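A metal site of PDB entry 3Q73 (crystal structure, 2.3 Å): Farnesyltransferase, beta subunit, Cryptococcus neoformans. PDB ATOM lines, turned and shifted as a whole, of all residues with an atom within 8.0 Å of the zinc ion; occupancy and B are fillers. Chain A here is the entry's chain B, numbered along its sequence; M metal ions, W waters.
The zinc ion is bound by NE2 of His 410 (2.0 Å).
OD2 of Asp 323 binds the zinc ion, at 2.2 Å.
The zinc ion is bound by water W1, at 2.4 Å.
The zinc ion is bound by SG of Cys 325.
The zinc ion has four donor atoms within binding distance.
Slightly farther from the zinc ion lies the side-chain carboxylate (OD1) of Asp 323 (2.7 Å).
CE2 of Tyr 409 touches the zinc ion, at 3.9 Å.
Within 4 Å of the zinc ion: Asp 323, Cys 325, Tyr 409 and His 410.
The nearest printed residue that does not touch the zinc ion is Asp 400 (4.2 Å).
N of His 410 sits at hydrogen-bond distance from OD1 of Asp 407.
The backbone carbonyl oxygen of His 410 sits close to the side-chain amide oxygen of Asn 414.
The side-chain sulfur (SG) of Cys 325 lies close to the side-chain hydroxyl (OH) of Tyr 409 (3.6 Å).
The side-chain hydroxyl (OH) of Tyr 409 is in hydrogen-bond range of the indole nitrogen (NE1) of Trp 329.
N of Tyr 409 lies close to OD1 of Asp 407, 3.4 Å away.
O of Tyr 409 lies within hydrogen-bond range of ND2 of Asn 413 (3.0 Å).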
ATOM      1  N   LEU A 321     -21.396  16.808   7.269  1.00  0.00           N
ATOM      2  CA  LEU A 321     -20.459  16.744   8.379  1.00  0.00           C
ATOM      3  C   LEU A 321     -19.480  15.597   8.227  1.00  0.00           C
ATOM      4  O   LEU A 321     -19.825  14.522   7.721  1.00  0.00           O
ATOM      5  CB  LEU A 321     -21.214  16.625   9.704  1.00  0.00           C
ATOM      6  CG  LEU A 321     -22.255  17.715  10.031  1.00  0.00           C
ATOM      7  CD1 LEU A 321     -23.006  17.402  11.327  1.00  0.00           C
ATOM      8  CD2 LEU A 321     -21.621  19.106  10.082  1.00  0.00           C
ATOM      9  N   VAL A 322     -18.235  15.825   8.652  1.00  0.00           N
ATOM     10  CA  VAL A 322     -17.247  14.755   8.720  1.00  0.00           C
ATOM     11  C   VAL A 322     -17.720  13.651   9.661  1.00  0.00           C
ATOM     12  O   VAL A 322     -18.505  13.889  10.587  1.00  0.00           O
ATOM     13  CB  VAL A 322     -15.850  15.259   9.140  1.00  0.00           C
ATOM     14  CG1 VAL A 322     -15.294  16.214   8.096  1.00  0.00           C
ATOM     15  CG2 VAL A 322     -15.906  15.919  10.512  1.00  0.00           C
ATOM     16  N   ASP A 323     -17.259  12.429   9.393  1.00  0.00           N
ATOM     17  CA  ASP A 323     -17.700  11.252  10.134  1.00  0.00           C
ATOM     18  C   ASP A 323     -16.611  10.204  10.076  1.00  0.00           C
ATOM     19  O   ASP A 323     -16.153   9.820   9.001  1.00  0.00           O
ATOM     20  CB  ASP A 323     -18.997  10.718   9.517  1.00  0.00           C
ATOM     21  CG  ASP A 323     -19.542   9.488  10.227  1.00  0.00           C
ATOM     22  OD1 ASP A 323     -18.769   8.699  10.841  1.00  0.00           O
ATOM     23  OD2 ASP A 323     -20.765   9.290  10.162  1.00  0.00           O
ATOM     24  N   GLY A 324     -16.206   9.750  11.263  1.00  0.00           N
ATOM     25  CA  GLY A 324     -15.172   8.722  11.392  1.00  0.00           C
ATOM     26  C   GLY A 324     -15.304   7.554  10.429  1.00  0.00           C
ATOM     27  O   GLY A 324     -14.289   7.070   9.926  1.00  0.00           O
ATOM     28  N   CYS A 325     -16.534   7.113  10.147  1.00  0.00           N
ATOM     29  CA  CYS A 325     -16.739   5.914   9.305  1.00  0.00           C
ATOM     30  C   CYS A 325     -16.278   6.106   7.860  1.00  0.00           C
ATOM     31  O   CYS A 325     -15.902   5.142   7.197  1.00  0.00           O
ATOM     32  CB  CYS A 325     -18.188   5.397   9.361  1.00  0.00           C
ATOM     33  SG  CYS A 325     -19.460   6.430   8.561  1.00  0.00           S
ATOM     34  N   TYR A 326     -16.281   7.352   7.386  1.00  0.00           N
ATOM     35  CA  TYR A 326     -15.810   7.639   6.038  1.00  0.00           C
ATOM     36  C   TYR A 326     -14.297   7.565   5.893  1.00  0.00           C
ATOM     37  O   TYR A 326     -13.767   7.721   4.787  1.00  0.00           O
ATOM     38  CB  TYR A 326     -16.386   8.965   5.519  1.00  0.00           C
ATOM     39  CG  TYR A 326     -17.880   8.907   5.419  1.00  0.00           C
ATOM     40  CD1 TYR A 326     -18.500   7.984   4.564  1.00  0.00           C
ATOM     41  CD2 TYR A 326     -18.685   9.718   6.197  1.00  0.00           C
ATOM     42  CE1 TYR A 326     -19.876   7.890   4.486  1.00  0.00           C
ATOM     43  CE2 TYR A 326     -20.072   9.646   6.125  1.00  0.00           C
ATOM     44  CZ  TYR A 326     -20.652   8.730   5.259  1.00  0.00           C
ATOM     45  OH  TYR A 326     -22.016   8.641   5.184  1.00  0.00           O
ATOM     46  N   TRP A 329     -14.654   4.303   4.087  1.00  0.00           N
ATOM     47  CA  TRP A 329     -15.394   4.401   2.826  1.00  0.00           C
ATOM     48  C   TRP A 329     -14.705   5.307   1.796  1.00  0.00           C
ATOM     49  O   TRP A 329     -14.509   4.901   0.649  1.00  0.00           O
ATOM     50  CB  TRP A 329     -16.854   4.835   3.040  1.00  0.00           C
ATOM     51  CG  TRP A 329     -17.656   3.923   3.943  1.00  0.00           C
ATOM     52  CD1 TRP A 329     -18.307   4.277   5.087  1.00  0.00           C
ATOM     53  CD2 TRP A 329     -17.892   2.512   3.768  1.00  0.00           C
ATOM     54  NE1 TRP A 329     -18.930   3.187   5.648  1.00  0.00           N
ATOM     55  CE2 TRP A 329     -18.698   2.094   4.854  1.00  0.00           C
ATOM     56  CE3 TRP A 329     -17.509   1.559   2.811  1.00  0.00           C
ATOM     57  CZ2 TRP A 329     -19.124   0.752   5.015  1.00  0.00           C
ATOM     58  CZ3 TRP A 329     -17.924   0.233   2.967  1.00  0.00           C
ATOM     59  CH2 TRP A 329     -18.727  -0.158   4.062  1.00  0.00           C
ATOM     60  N   ARG A 399     -16.054   6.228  17.290  1.00  0.00           N
ATOM     61  CA  ARG A 399     -17.326   6.874  16.992  1.00  0.00           C
ATOM     62  C   ARG A 399     -17.333   7.720  15.724  1.00  0.00           C
ATOM     63  O   ARG A 399     -16.273   8.042  15.166  1.00  0.00           O
ATOM     64  CB  ARG A 399     -17.762   7.748  18.186  1.00  0.00           C
ATOM     65  CG  ARG A 399     -16.885   8.975  18.359  1.00  0.00           C
ATOM     66  CD  ARG A 399     -16.923   9.514  19.751  1.00  0.00           C
ATOM     67  NE  ARG A 399     -15.832  10.456  19.944  1.00  0.00           N
ATOM     68  CZ  ARG A 399     -15.589  11.122  21.078  1.00  0.00           C
ATOM     69  NH1 ARG A 399     -16.366  10.947  22.145  1.00  0.00           N
ATOM     70  NH2 ARG A 399     -14.556  11.955  21.143  1.00  0.00           N
ATOM     71  N   ASP A 400     -18.540   8.079  15.297  1.00  0.00           N
ATOM     72  CA  ASP A 400     -18.763   9.028  14.203  1.00  0.00           C
ATOM     73  C   ASP A 400     -18.031  10.360  14.450  1.00  0.00           C
ATOM     74  O   ASP A 400     -17.177  10.755  13.668  1.00  0.00           O
ATOM     75  CB  ASP A 400     -20.280   9.187  14.020  1.00  0.00           C
ATOM     76  CG  ASP A 400     -20.683  10.494  13.336  1.00  0.00           C
ATOM     77  OD1 ASP A 400     -19.844  11.221  12.758  1.00  0.00           O
ATOM     78  OD2 ASP A 400     -21.900  10.779  13.372  1.00  0.00           O
ATOM     79  N   LYS A 401     -18.357  11.023  15.563  1.00  0.00           N
ATOM     80  CA  LYS A 401     -17.722  12.279  15.938  1.00  0.00           C
ATOM     81  C   LYS A 401     -17.947  12.554  17.431  1.00  0.00           C
ATOM     82  O   LYS A 401     -18.776  11.891  18.060  1.00  0.00           O
ATOM     83  CB  LYS A 401     -18.232  13.441  15.072  1.00  0.00           C
ATOM     84  CG  LYS A 401     -19.727  13.663  15.101  1.00  0.00           C
ATOM     85  CD  LYS A 401     -20.158  14.898  14.305  1.00  0.00           C
ATOM     86  CE  LYS A 401     -20.218  14.634  12.814  1.00  0.00           C
ATOM     87  NZ  LYS A 401     -21.264  13.632  12.445  1.00  0.00           N
ATOM     88  N   ASP A 407     -19.974   2.844  18.501  1.00  0.00           N
ATOM     89  CA  ASP A 407     -20.602   1.559  18.234  1.00  0.00           C
ATOM     90  C   ASP A 407     -19.676   0.636  17.456  1.00  0.00           C
ATOM     91  O   ASP A 407     -18.573   1.041  17.063  1.00  0.00           O
ATOM     92  CB  ASP A 407     -21.974   1.707  17.549  1.00  0.00           C
ATOM     93  CG  ASP A 407     -21.911   2.453  16.217  1.00  0.00           C
ATOM     94  OD1 ASP A 407     -20.840   2.479  15.575  1.00  0.00           O
ATOM     95  OD2 ASP A 407     -22.953   2.984  15.804  1.00  0.00           O
ATOM     96  N   TYR A 409     -20.020  -0.619  14.439  1.00  0.00           N
ATOM     97  CA  TYR A 409     -19.886  -0.153  13.072  1.00  0.00           C
ATOM     98  C   TYR A 409     -18.793   0.911  12.912  1.00  0.00           C
ATOM     99  O   TYR A 409     -17.930   0.794  12.046  1.00  0.00           O
ATOM    100  CB  TYR A 409     -21.233   0.386  12.554  1.00  0.00           C
ATOM    101  CG  TYR A 409     -21.153   1.162  11.264  1.00  0.00           C
ATOM    102  CD1 TYR A 409     -21.080   0.506  10.035  1.00  0.00           C
ATOM    103  CD2 TYR A 409     -21.139   2.561  11.260  1.00  0.00           C
ATOM    104  CE1 TYR A 409     -21.009   1.198   8.845  1.00  0.00           C
ATOM    105  CE2 TYR A 409     -21.067   3.277  10.065  1.00  0.00           C
ATOM    106  CZ  TYR A 409     -20.996   2.591   8.857  1.00  0.00           C
ATOM    107  OH  TYR A 409     -20.917   3.280   7.674  1.00  0.00           O
ATOM    108  N   HIS A 410     -18.852   1.957  13.740  1.00  0.00           N
ATOM    109  CA  HIS A 410     -17.873   3.034  13.673  1.00  0.00           C
ATOM    110  C   HIS A 410     -16.494   2.622  14.179  1.00  0.00           C
ATOM    111  O   HIS A 410     -15.474   3.108  13.679  1.00  0.00           O
ATOM    112  CB  HIS A 410     -18.386   4.282  14.387  1.00  0.00           C
ATOM    113  CG  HIS A 410     -19.448   5.011  13.619  1.00  0.00           C
ATOM    114  ND1 HIS A 410     -20.792   4.848  13.859  1.00  0.00           N
ATOM    115  CD2 HIS A 410     -19.351   5.883  12.579  1.00  0.00           C
ATOM    116  CE1 HIS A 410     -21.484   5.597  13.018  1.00  0.00           C
ATOM    117  NE2 HIS A 410     -20.628   6.232  12.232  1.00  0.00           N
ATOM    118  N   ASN A 413     -14.992   0.685  11.184  1.00  0.00           N
ATOM    119  CA  ASN A 413     -14.685   1.554  10.056  1.00  0.00           C
ATOM    120  C   ASN A 413     -13.641   2.624  10.330  1.00  0.00           C
ATOM    121  O   ASN A 413     -12.862   2.981   9.441  1.00  0.00           O
ATOM    122  CB  ASN A 413     -15.976   2.109   9.447  1.00  0.00           C
ATOM    123  CG  ASN A 413     -16.759   1.035   8.700  1.00  0.00           C
ATOM    124  OD1 ASN A 413     -16.214   0.373   7.830  1.00  0.00           O
ATOM    125  ND2 ASN A 413     -18.014   0.857   9.070  1.00  0.00           N
ATOM    126  N   ASN A 414     -13.617   3.125  11.567  1.00  0.00           N
ATOM    127  CA  ASN A 414     -12.519   3.997  11.994  1.00  0.00           C
ATOM    128  C   ASN A 414     -11.183   3.259  11.931  1.00  0.00           C
ATOM    129  O   ASN A 414     -10.211   3.771  11.371  1.00  0.00           O
ATOM    130  CB  ASN A 414     -12.754   4.530  13.407  1.00  0.00           C
ATOM    131  CG  ASN A 414     -13.548   5.814  13.419  1.00  0.00           C
ATOM    132  OD1 ASN A 414     -14.707   5.842  13.834  1.00  0.00           O
ATOM    133  ND2 ASN A 414     -12.936   6.887  12.961  1.00  0.00           N
HETATM  134 ZN    ZN M   1     -20.918   7.138  10.420  1.00  0.00          ZN
HETATM  135  O   HOH W   1     -23.315   6.797  10.289  1.00  0.00           O
